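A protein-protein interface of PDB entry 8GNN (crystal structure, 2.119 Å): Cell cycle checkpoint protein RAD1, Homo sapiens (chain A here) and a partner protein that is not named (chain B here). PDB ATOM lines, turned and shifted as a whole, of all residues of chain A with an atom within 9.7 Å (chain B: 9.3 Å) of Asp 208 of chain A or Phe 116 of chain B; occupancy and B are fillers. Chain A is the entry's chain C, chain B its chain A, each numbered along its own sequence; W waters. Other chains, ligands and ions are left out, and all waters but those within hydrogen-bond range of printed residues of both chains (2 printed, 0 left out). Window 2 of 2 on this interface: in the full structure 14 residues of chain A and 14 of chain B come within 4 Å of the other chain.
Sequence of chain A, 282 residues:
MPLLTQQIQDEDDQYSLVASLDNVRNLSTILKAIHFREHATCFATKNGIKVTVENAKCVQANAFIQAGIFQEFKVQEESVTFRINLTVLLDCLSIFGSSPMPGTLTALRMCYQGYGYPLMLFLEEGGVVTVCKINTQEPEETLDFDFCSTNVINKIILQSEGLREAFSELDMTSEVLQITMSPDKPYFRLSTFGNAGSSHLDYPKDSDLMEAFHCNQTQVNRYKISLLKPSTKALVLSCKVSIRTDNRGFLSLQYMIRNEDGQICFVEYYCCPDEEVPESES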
ATOM      1  N   ILE A 157      10.823 -39.420  20.253  1.00  0.00           N
ATOM      2  CA  ILE A 157      12.116 -39.147  20.867  1.00  0.00           C
ATOM      3  C   ILE A 157      12.784 -37.961  20.179  1.00  0.00           C
ATOM      4  O   ILE A 157      12.995 -37.973  18.966  1.00  0.00           O
ATOM      5  CB  ILE A 157      13.043 -40.372  20.809  1.00  0.00           C
ATOM      6  CG1 ILE A 157      12.460 -41.514  21.644  1.00  0.00           C
ATOM      7  CG2 ILE A 157      14.433 -40.010  21.305  1.00  0.00           C
ATOM      8  CD1 ILE A 157      13.300 -42.771  21.633  1.00  0.00           C
ATOM      9  N   LEU A 158      13.111 -36.939  20.963  1.00  0.00           N
ATOM     10  CA  LEU A 158      13.653 -35.698  20.422  1.00  0.00           C
ATOM     11  C   LEU A 158      15.021 -35.352  20.997  1.00  0.00           C
ATOM     12  O   LEU A 158      15.326 -35.676  22.145  1.00  0.00           O
ATOM     13  CB  LEU A 158      12.692 -34.538  20.691  1.00  0.00           C
ATOM     14  CG  LEU A 158      11.368 -34.516  19.930  1.00  0.00           C
ATOM     15  CD1 LEU A 158      10.309 -33.805  20.749  1.00  0.00           C
ATOM     16  CD2 LEU A 158      11.546 -33.837  18.583  1.00  0.00           C
ATOM     17  N   GLN A 159      15.838 -34.689  20.186  1.00  0.00           N
ATOM     18  CA  GLN A 159      17.072 -34.093  20.676  1.00  0.00           C
ATOM     19  C   GLN A 159      16.705 -32.927  21.586  1.00  0.00           C
ATOM     20  O   GLN A 159      16.014 -31.999  21.165  1.00  0.00           O
ATOM     21  CB  GLN A 159      17.956 -33.629  19.520  1.00  0.00           C
ATOM     22  CG  GLN A 159      18.482 -34.762  18.654  1.00  0.00           C
ATOM     23  CD  GLN A 159      19.245 -34.267  17.443  1.00  0.00           C
ATOM     24  OE1 GLN A 159      19.616 -33.096  17.364  1.00  0.00           O
ATOM     25  NE2 GLN A 159      19.485 -35.161  16.488  1.00  0.00           N
ATOM     26  N   SER A 160      17.161 -32.984  22.831  1.00  0.00           N
ATOM     27  CA  SER A 160      16.733 -32.029  23.848  1.00  0.00           C
ATOM     28  C   SER A 160      17.167 -30.596  23.554  1.00  0.00           C
ATOM     29  O   SER A 160      16.439 -29.653  23.857  1.00  0.00           O
ATOM     30  CB  SER A 160      17.259 -32.455  25.220  1.00  0.00           C
ATOM     31  OG  SER A 160      16.642 -33.659  25.646  1.00  0.00           O
ATOM     32  N   GLU A 161      18.347 -30.439  22.959  1.00  0.00           N
ATOM     33  CA  GLU A 161      18.923 -29.117  22.714  1.00  0.00           C
ATOM     34  C   GLU A 161      18.028 -28.218  21.861  1.00  0.00           C
ATOM     35  O   GLU A 161      17.906 -27.023  22.127  1.00  0.00           O
ATOM     36  CB  GLU A 161      20.295 -29.255  22.050  1.00  0.00           C
ATOM     37  CG  GLU A 161      21.452 -28.758  22.906  1.00  0.00           C
ATOM     38  CD  GLU A 161      21.550 -27.244  22.931  1.00  0.00           C
ATOM     39  OE1 GLU A 161      20.995 -26.596  22.019  1.00  0.00           O
ATOM     40  OE2 GLU A 161      22.180 -26.703  23.864  1.00  0.00           O
ATOM     41  N   GLY A 162      17.399 -28.796  20.843  1.00  0.00           N
ATOM     42  CA  GLY A 162      16.556 -28.031  19.941  1.00  0.00           C
ATOM     43  C   GLY A 162      15.177 -27.719  20.495  1.00  0.00           C
ATOM     44  O   GLY A 162      14.371 -27.060  19.838  1.00  0.00           O
ATOM     45  N   LEU A 163      14.906 -28.190  21.708  1.00  0.00           N
ATOM     46  CA  LEU A 163      13.603 -28.002  22.337  1.00  0.00           C
ATOM     47  C   LEU A 163      13.737 -27.272  23.676  1.00  0.00           C
ATOM     48  O   LEU A 163      12.766 -26.715  24.191  1.00  0.00           O
ATOM     49  CB  LEU A 163      12.912 -29.362  22.522  1.00  0.00           C
ATOM     50  CG  LEU A 163      11.716 -29.533  23.467  1.00  0.00           C
ATOM     51  CD1 LEU A 163      10.533 -28.672  23.048  1.00  0.00           C
ATOM     52  CD2 LEU A 163      11.309 -30.996  23.544  1.00  0.00           C
ATOM     53  N   TYR A 187       1.892 -33.307  13.008  1.00  0.00           N
ATOM     54  CA  TYR A 187       2.763 -34.358  13.547  1.00  0.00           C
ATOM     55  C   TYR A 187       2.986 -34.233  15.056  1.00  0.00           C
ATOM     56  O   TYR A 187       2.563 -35.101  15.820  1.00  0.00           O
ATOM     57  CB  TYR A 187       4.105 -34.366  12.809  1.00  0.00           C
ATOM     58  CG  TYR A 187       3.957 -34.523  11.312  1.00  0.00           C
ATOM     59  CD1 TYR A 187       3.162 -35.529  10.779  1.00  0.00           C
ATOM     60  CD2 TYR A 187       4.590 -33.653  10.435  1.00  0.00           C
ATOM     61  CE1 TYR A 187       3.014 -35.674   9.412  1.00  0.00           C
ATOM     62  CE2 TYR A 187       4.448 -33.790   9.066  1.00  0.00           C
ATOM     63  CZ  TYR A 187       3.659 -34.802   8.560  1.00  0.00           C
ATOM     64  OH  TYR A 187       3.512 -34.944   7.200  1.00  0.00           O
ATOM     65  N   ASP A 202       5.212 -26.302  16.599  1.00  0.00           N
ATOM     66  CA  ASP A 202       5.106 -27.494  15.763  1.00  0.00           C
ATOM     67  C   ASP A 202       6.455 -28.089  15.371  1.00  0.00           C
ATOM     68  O   ASP A 202       7.370 -27.377  14.958  1.00  0.00           O
ATOM     69  CB  ASP A 202       4.307 -27.177  14.497  1.00  0.00           C
ATOM     70  CG  ASP A 202       2.877 -26.777  14.796  1.00  0.00           C
ATOM     71  OD1 ASP A 202       2.427 -26.993  15.939  1.00  0.00           O
ATOM     72  OD2 ASP A 202       2.201 -26.253  13.886  1.00  0.00           O
ATOM     73  N   TYR A 203       6.559 -29.409  15.498  1.00  0.00           N
ATOM     74  CA  TYR A 203       7.740 -30.146  15.070  1.00  0.00           C
ATOM     75  C   TYR A 203       7.362 -31.167  14.003  1.00  0.00           C
ATOM     76  O   TYR A 203       6.582 -32.082  14.268  1.00  0.00           O
ATOM     77  CB  TYR A 203       8.403 -30.849  16.257  1.00  0.00           C
ATOM     78  CG  TYR A 203       8.960 -29.911  17.302  1.00  0.00           C
ATOM     79  CD1 TYR A 203       8.146 -29.382  18.296  1.00  0.00           C
ATOM     80  CD2 TYR A 203      10.304 -29.561  17.301  1.00  0.00           C
ATOM     81  CE1 TYR A 203       8.654 -28.526  19.253  1.00  0.00           C
ATOM     82  CE2 TYR A 203      10.820 -28.706  18.255  1.00  0.00           C
ATOM     83  CZ  TYR A 203       9.991 -28.191  19.228  1.00  0.00           C
ATOM     84  OH  TYR A 203      10.503 -27.338  20.178  1.00  0.00           O
ATOM     85  N   PRO A 204       7.908 -31.011  12.788  1.00  0.00           N
ATOM     86  CA  PRO A 204       7.629 -31.971  11.717  1.00  0.00           C
ATOM     87  C   PRO A 204       8.330 -33.300  11.975  1.00  0.00           C
ATOM     88  O   PRO A 204       9.402 -33.313  12.578  1.00  0.00           O
ATOM     89  CB  PRO A 204       8.187 -31.278  10.473  1.00  0.00           C
ATOM     90  CG  PRO A 204       9.285 -30.418  10.996  1.00  0.00           C
ATOM     91  CD  PRO A 204       8.835 -29.951  12.357  1.00  0.00           C
ATOM     92  N   LYS A 205       7.735 -34.400  11.529  1.00  0.00           N
ATOM     93  CA  LYS A 205       8.285 -35.723  11.807  1.00  0.00           C
ATOM     94  C   LYS A 205       9.588 -35.974  11.050  1.00  0.00           C
ATOM     95  O   LYS A 205      10.357 -36.864  11.410  1.00  0.00           O
ATOM     96  CB  LYS A 205       7.265 -36.811  11.466  1.00  0.00           C
ATOM     97  CG  LYS A 205       6.944 -36.927   9.988  1.00  0.00           C
ATOM     98  CD  LYS A 205       6.007 -38.092   9.722  1.00  0.00           C
ATOM     99  CE  LYS A 205       5.763 -38.276   8.234  1.00  0.00           C
ATOM    100  NZ  LYS A 205       4.852 -39.421   7.959  1.00  0.00           N
ATOM    101  N   ASP A 206       9.834 -35.187  10.008  1.00  0.00           N
ATOM    102  CA  ASP A 206      11.048 -35.341   9.212  1.00  0.00           C
ATOM    103  C   ASP A 206      12.207 -34.520   9.773  1.00  0.00           C
ATOM    104  O   ASP A 206      13.316 -34.550   9.239  1.00  0.00           O
ATOM    105  CB  ASP A 206      10.788 -34.952   7.750  1.00  0.00           C
ATOM    106  CG  ASP A 206      10.300 -33.516   7.594  1.00  0.00           C
ATOM    107  OD1 ASP A 206      10.320 -32.749   8.578  1.00  0.00           O
ATOM    108  OD2 ASP A 206       9.900 -33.152   6.468  1.00  0.00           O
ATOM    109  N   SER A 207      11.940 -33.786  10.850  1.00  0.00           N
ATOM    110  CA  SER A 207      12.924 -32.878  11.431  1.00  0.00           C
ATOM    111  C   SER A 207      14.165 -33.606  11.935  1.00  0.00           C
ATOM    112  O   SER A 207      14.093 -34.760  12.357  1.00  0.00           O
ATOM    113  CB  SER A 207      12.298 -32.078  12.575  1.00  0.00           C
ATOM    114  OG  SER A 207      13.265 -31.270  13.223  1.00  0.00           O
ATOM    115  N   ASP A 208      15.302 -32.919  11.889  1.00  0.00           N
ATOM    116  CA  ASP A 208      16.557 -33.470  12.388  1.00  0.00           C
ATOM    117  C   ASP A 208      16.523 -33.602  13.906  1.00  0.00           C
ATOM    118  O   ASP A 208      17.302 -34.352  14.493  1.00  0.00           O
ATOM    119  CB  ASP A 208      17.737 -32.598  11.959  1.00  0.00           C
ATOM    120  CG  ASP A 208      17.981 -32.641  10.463  1.00  0.00           C
ATOM    121  OD1 ASP A 208      17.357 -33.482   9.782  1.00  0.00           O
ATOM    122  OD2 ASP A 208      18.796 -31.834   9.969  1.00  0.00           O
ATOM    123  N   LEU A 209      15.617 -32.862  14.538  1.00  0.00           N
ATOM    124  CA  LEU A 209      15.423 -32.951  15.979  1.00  0.00           C
ATOM    125  C   LEU A 209      14.636 -34.207  16.331  1.00  0.00           C
ATOM    126  O   LEU A 209      14.664 -34.672  17.470  1.00  0.00           O
ATOM    127  CB  LEU A 209      14.700 -31.708  16.503  1.00  0.00           C
ATOM    128  CG  LEU A 209      15.382 -30.361  16.255  1.00  0.00           C
ATOM    129  CD1 LEU A 209      14.470 -29.214  16.661  1.00  0.00           C
ATOM    130  CD2 LEU A 209      16.708 -30.285  16.996  1.00  0.00           C
ATOM    131  N   MET A 210      13.936 -34.750  15.340  1.00  0.00           N
ATOM    132  CA  MET A 210      13.107 -35.934  15.530  1.00  0.00           C
ATOM    133  C   MET A 210      13.912 -37.211  15.308  1.00  0.00           C
ATOM    134  O   MET A 210      14.135 -37.620  14.169  1.00  0.00           O
ATOM    135  CB  MET A 210      11.908 -35.899  14.580  1.00  0.00           C
ATOM    136  CG  MET A 210      10.778 -36.838  14.957  1.00  0.00           C
ATOM    137  SD  MET A 210       9.812 -36.217  16.343  1.00  0.00           S
ATOM    138  CE  MET A 210       8.828 -34.955  15.536  1.00  0.00           C
ATOM    139  N   GLU A 211      14.346 -37.839  16.397  1.00  0.00           N
ATOM    140  CA  GLU A 211      15.150 -39.054  16.304  1.00  0.00           C
ATOM    141  C   GLU A 211      14.286 -40.304  16.175  1.00  0.00           C
ATOM    142  O   GLU A 211      14.700 -41.295  15.574  1.00  0.00           O
ATOM    143  CB  GLU A 211      16.069 -39.182  17.518  1.00  0.00           C
ATOM    144  CG  GLU A 211      17.258 -38.241  17.494  1.00  0.00           C
ATOM    145  CD  GLU A 211      18.306 -38.621  18.515  1.00  0.00           C
ATOM    146  OE1 GLU A 211      18.138 -39.671  19.170  1.00  0.00           O
ATOM    147  OE2 GLU A 211      19.300 -37.879  18.659  1.00  0.00           O
ATOM    148  N   ALA A 212      13.088 -40.257  16.747  1.00  0.00           N
ATOM    149  CA  ALA A 212      12.153 -41.368  16.647  1.00  0.00           C
ATOM    150  C   ALA A 212      10.718 -40.858  16.616  1.00  0.00           C
ATOM    151  O   ALA A 212      10.321 -40.043  17.448  1.00  0.00           O
ATOM    152  CB  ALA A 212      12.349 -42.339  17.801  1.00  0.00           C
ATOM    153  N   CYS A 239      20.056 -34.819  27.109  1.00  0.00           N
ATOM    154  CA  CYS A 239      20.529 -34.742  25.734  1.00  0.00           C
ATOM    155  C   CYS A 239      19.460 -35.295  24.799  1.00  0.00           C
ATOM    156  O   CYS A 239      19.401 -34.942  23.621  1.00  0.00           O
ATOM    157  CB  CYS A 239      21.843 -35.507  25.564  1.00  0.00           C
ATOM    158  SG  CYS A 239      21.762 -37.253  26.027  1.00  0.00           S
ATOM    159  N   LYS A 240      18.618 -36.170  25.339  1.00  0.00           N
ATOM    160  CA  LYS A 240      17.477 -36.708  24.607  1.00  0.00           C
ATOM    161  C   LYS A 240      16.242 -36.722  25.501  1.00  0.00           C
ATOM    162  O   LYS A 240      16.354 -36.820  26.722  1.00  0.00           O
ATOM    163  CB  LYS A 240      17.767 -38.120  24.094  1.00  0.00           C
ATOM    164  CG  LYS A 240      18.903 -38.212  23.090  1.00  0.00           C
ATOM    165  CD  LYS A 240      19.020 -39.619  22.528  1.00  0.00           C
ATOM    166  CE  LYS A 240      20.192 -39.738  21.570  1.00  0.00           C
ATOM    167  NZ  LYS A 240      20.195 -41.050  20.868  1.00  0.00           N
ATOM    168  N   LYS B  92      19.626 -17.115  16.486  1.00  0.00           N
ATOM    169  CA  LYS B  92      20.112 -18.480  16.317  1.00  0.00           C
ATOM    170  C   LYS B  92      19.068 -19.417  15.709  1.00  0.00           C
ATOM    171  O   LYS B  92      19.405 -20.307  14.931  1.00  0.00           O
ATOM    172  CB  LYS B  92      20.585 -19.042  17.662  1.00  0.00           C
ATOM    173  CG  LYS B  92      21.210 -20.430  17.577  1.00  0.00           C
ATOM    174  CD  LYS B  92      22.257 -20.501  16.473  1.00  0.00           C
ATOM    175  CE  LYS B  92      23.038 -21.805  16.525  1.00  0.00           C
ATOM    176  NZ  LYS B  92      24.256 -21.753  15.670  1.00  0.00           N
ATOM    177  N   THR B  93      17.802 -19.212  16.056  1.00  0.00           N
ATOM    178  CA  THR B  93      16.767 -20.181  15.709  1.00  0.00           C
ATOM    179  C   THR B  93      15.822 -19.704  14.605  1.00  0.00           C
ATOM    180  O   THR B  93      15.480 -20.469  13.703  1.00  0.00           O
ATOM    181  CB  THR B  93      15.934 -20.553  16.951  1.00  0.00           C
ATOM    182  OG1 THR B  93      16.809 -20.946  18.014  1.00  0.00           O
ATOM    183  CG2 THR B  93      14.988 -21.697  16.637  1.00  0.00           C
ATOM    184  N   VAL B  94      15.401 -18.445  14.673  1.00  0.00           N
ATOM    185  CA  VAL B  94      14.406 -17.931  13.735  1.00  0.00           C
ATOM    186  C   VAL B  94      15.019 -17.528  12.396  1.00  0.00           C
ATOM    187  O   VAL B  94      15.936 -16.709  12.340  1.00  0.00           O
ATOM    188  CB  VAL B  94      13.656 -16.722  14.324  1.00  0.00           C
ATOM    189  CG1 VAL B  94      12.583 -16.244  13.357  1.00  0.00           C
ATOM    190  CG2 VAL B  94      13.045 -17.086  15.666  1.00  0.00           C
ATOM    191  N   GLU B  95      14.501 -18.111  11.319  1.00  0.00           N
ATOM    192  CA  GLU B  95      14.968 -17.804   9.972  1.00  0.00           C
ATOM    193  C   GLU B  95      14.046 -16.799   9.287  1.00  0.00           C
ATOM    194  O   GLU B  95      14.508 -15.886   8.603  1.00  0.00           O
ATOM    195  CB  GLU B  95      15.070 -19.082   9.137  1.00  0.00           C
ATOM    196  CG  GLU B  95      16.127 -20.059   9.631  1.00  0.00           C
ATOM    197  CD  GLU B  95      16.121 -21.367   8.863  1.00  0.00           C
ATOM    198  OE1 GLU B  95      15.156 -21.613   8.110  1.00  0.00           O
ATOM    199  OE2 GLU B  95      17.084 -22.148   9.014  1.00  0.00           O
ATOM    200  N   HIS B 113       9.293 -19.011  11.443  1.00  0.00           N
ATOM    201  CA  HIS B 113       9.847 -20.169  10.757  1.00  0.00           C
ATOM    202  C   HIS B 113      11.259 -20.417  11.269  1.00  0.00           C
ATOM    203  O   HIS B 113      12.174 -19.637  11.004  1.00  0.00           O
ATOM    204  CB  HIS B 113       9.841 -19.960   9.243  1.00  0.00           C
ATOM    205  CG  HIS B 113       8.477 -19.725   8.674  1.00  0.00           C
ATOM    206  ND1 HIS B 113       7.644 -20.752   8.287  1.00  0.00           N
ATOM    207  CD2 HIS B 113       7.797 -18.580   8.433  1.00  0.00           C
ATOM    208  CE1 HIS B 113       6.512 -20.251   7.829  1.00  0.00           C
ATOM    209  NE2 HIS B 113       6.578 -18.934   7.907  1.00  0.00           N
ATOM    210  N   CYS B 114      11.428 -21.504  12.014  1.00  0.00           N
ATOM    211  CA  CYS B 114      12.678 -21.754  12.716  1.00  0.00           C
ATOM    212  C   CYS B 114      13.481 -22.892  12.098  1.00  0.00           C
ATOM    213  O   CYS B 114      13.029 -23.551  11.161  1.00  0.00           O
ATOM    214  CB  CYS B 114      12.395 -22.054  14.188  1.00  0.00           C
ATOM    215  SG  CYS B 114      11.395 -20.792  15.016  1.00  0.00           S
ATOM    216  N   LYS B 115      14.678 -23.112  12.633  1.00  0.00           N
ATOM    217  CA  LYS B 115      15.561 -24.163  12.144  1.00  0.00           C
ATOM    218  C   LYS B 115      14.956 -25.546  12.356  1.00  0.00           C
ATOM    219  O   LYS B 115      14.100 -25.733  13.221  1.00  0.00           O
ATOM    220  CB  LYS B 115      16.926 -24.077  12.829  1.00  0.00           C
ATOM    221  CG  LYS B 115      17.802 -22.943  12.326  1.00  0.00           C
ATOM    222  CD  LYS B 115      19.179 -22.982  12.965  1.00  0.00           C
ATOM    223  CE  LYS B 115      20.114 -21.974  12.316  1.00  0.00           C
ATOM    224  NZ  LYS B 115      21.487 -22.036  12.892  1.00  0.00           N
ATOM    225  N   PHE B 116      15.412 -26.501  11.549  1.00  0.00           N
ATOM    226  CA  PHE B 116      14.967 -27.892  11.622  1.00  0.00           C
ATOM    227  C   PHE B 116      13.461 -28.029  11.412  1.00  0.00           C
ATOM    228  O   PHE B 116      12.826 -28.921  11.973  1.00  0.00           O
ATOM    229  CB  PHE B 116      15.373 -28.515  12.960  1.00  0.00           C
ATOM    230  CG  PHE B 116      16.786 -28.206  13.366  1.00  0.00           C
ATOM    231  CD1 PHE B 116      17.855 -28.694  12.631  1.00  0.00           C
ATOM    232  CD2 PHE B 116      17.046 -27.429  14.483  1.00  0.00           C
ATOM    233  CE1 PHE B 116      19.156 -28.409  13.003  1.00  0.00           C
ATOM    234  CE2 PHE B 116      18.344 -27.142  14.860  1.00  0.00           C
ATOM    235  CZ  PHE B 116      19.401 -27.633  14.118  1.00  0.00           C
ATOM    236  N   GLY B 117      12.896 -27.138  10.603  1.00  0.00           N
ATOM    237  CA  GLY B 117      11.497 -27.221  10.222  1.00  0.00           C
ATOM    238  C   GLY B 117      10.505 -26.845  11.308  1.00  0.00           C
ATOM    239  O   GLY B 117       9.296 -26.969  11.117  1.00  0.00           O
ATOM    240  N   VAL B 118      11.011 -26.385  12.447  1.00  0.00           N
ATOM    241  CA  VAL B 118      10.148 -25.989  13.555  1.00  0.00           C
ATOM    242  C   VAL B 118       9.412 -24.691  13.235  1.00  0.00           C
ATOM    243  O   VAL B 118      10.012 -23.731  12.751  1.00  0.00           O
ATOM    244  CB  VAL B 118      10.950 -25.812  14.858  1.00  0.00           C
ATOM    245  CG1 VAL B 118      10.023 -25.462  16.014  1.00  0.00           C
ATOM    246  CG2 VAL B 118      11.738 -27.075  15.167  1.00  0.00           C
ATOM    247  N   ARG B 119       8.110 -24.669  13.498  1.00  0.00           N
ATOM    248  CA  ARG B 119       7.308 -23.474  13.265  1.00  0.00           C
ATOM    249  C   ARG B 119       6.551 -23.075  14.528  1.00  0.00           C
ATOM    250  O   ARG B 119       5.854 -23.894  15.129  1.00  0.00           O
ATOM    251  CB  ARG B 119       6.329 -23.696  12.109  1.00  0.00           C
ATOM    252  CG  ARG B 119       5.688 -22.419  11.585  1.00  0.00           C
ATOM    253  CD  ARG B 119       4.879 -22.669  10.319  1.00  0.00           C
ATOM    254  NE  ARG B 119       3.588 -23.293  10.597  1.00  0.00           N
ATOM    255  CZ  ARG B 119       2.684 -23.584   9.667  1.00  0.00           C
ATOM    256  NH1 ARG B 119       2.929 -23.309   8.393  1.00  0.00           N
ATOM    257  NH2 ARG B 119       1.535 -24.149  10.010  1.00  0.00           N
HETATM  258  O   HOH W   1       3.050 -26.372  11.144  1.00  0.00           O
HETATM  259  O   HOH W   2       3.257 -23.395  14.546  1.00  0.00           O
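The backbone carbonyl oxygen (O) of Phe 116 of chain B lies within hydrogen-bond range of the side-chain hydroxyl (OG) of Ser 207 of chain A, 2.7 Å away.
O of Arg 119 of chain B sits at hydrogen-bond distance from N of Asp 202 of chain A (2.9 Å).
Leu 209 of chain A touches just these residues of chain B: Phe 116 (3.8 Å) and Val 118 (3.8 Å).
Gly 117 of chain B touches one residue of chain A.
Of the printed residues of chain B, Asp 202 of chain A touches Val 118 (3.4 Å) and Arg 119 (2.9 Å).
Of the printed residues of chain A, Val 118 of chain B touches Asp 202, Tyr 203 and Leu 209.
Of the printed residues of chain B, Pro 204 of chain A touches Phe 116 and Gly 117.
Leu 158 of chain A touches none of the printed residues of chain B.
Ala 212 of chain A touches none of the printed residues of chain B.
The nearest residue of chain B that does not touch Asp 208 of chain A is Gly 117 of chain B (6.4 Å).
The nearest printed residue of chain B that does not touch Asp 202 of chain A is Gly 117 of chain B (4.3 Å).
Among the printed residues, pairs that only touch across the chains: Asp 202 of chain A with Val 118 of chain B (3.4 Å), Tyr 203 of chain A with Val 118 of chain B (3.6 Å), Pro 204 of chain A with Phe 116 of chain B (3.97 Å), Pro 204 of chain A with Gly 117 of chain B (3.3 Å), Asp 208 of chain A with Phe 116 of chain B (3.96 Å), Leu 209 of chain A with Phe 116 of chain B (3.8 Å) and Leu 209 of chain A with Val 118 of chain B (3.8 Å).
The side-chain amide nitrogen (NE2) of Gln 159 of chain A is in hydrogen-bond range of the backbone carbonyl oxygen (O) of Asp 208 of chain A (3.1 Å).
The backbone carbonyl oxygen (O) of Leu 209 of chain A lies within hydrogen-bond range of the backbone NH (N) of Gln 159 of chain A (3.0 Å).
The side-chain hydroxyl of Ser 207 of chain A lies close to the backbone NH of Leu 209 of chain A (3.1 Å).
Of the 21 printed residues of chain A, 6 touch a printed residue of chain B.
Hydrophobic or aromatic side chains of chain A within 4 Å of the printed part of chain B: Tyr 203, Pro 204 and Leu 209.
Water W2 lies within hydrogen-bond range of O of Arg 119 of chain B (2.7 Å) and OD2 of Asp 202 of chain A (3.1 Å).
Water W1 lies within hydrogen-bond range of the side-chain carboxylate of Asp 202 of chain A (2.9 Å) and the guanidinium group of Arg 119 of chain B (2.9 Å).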
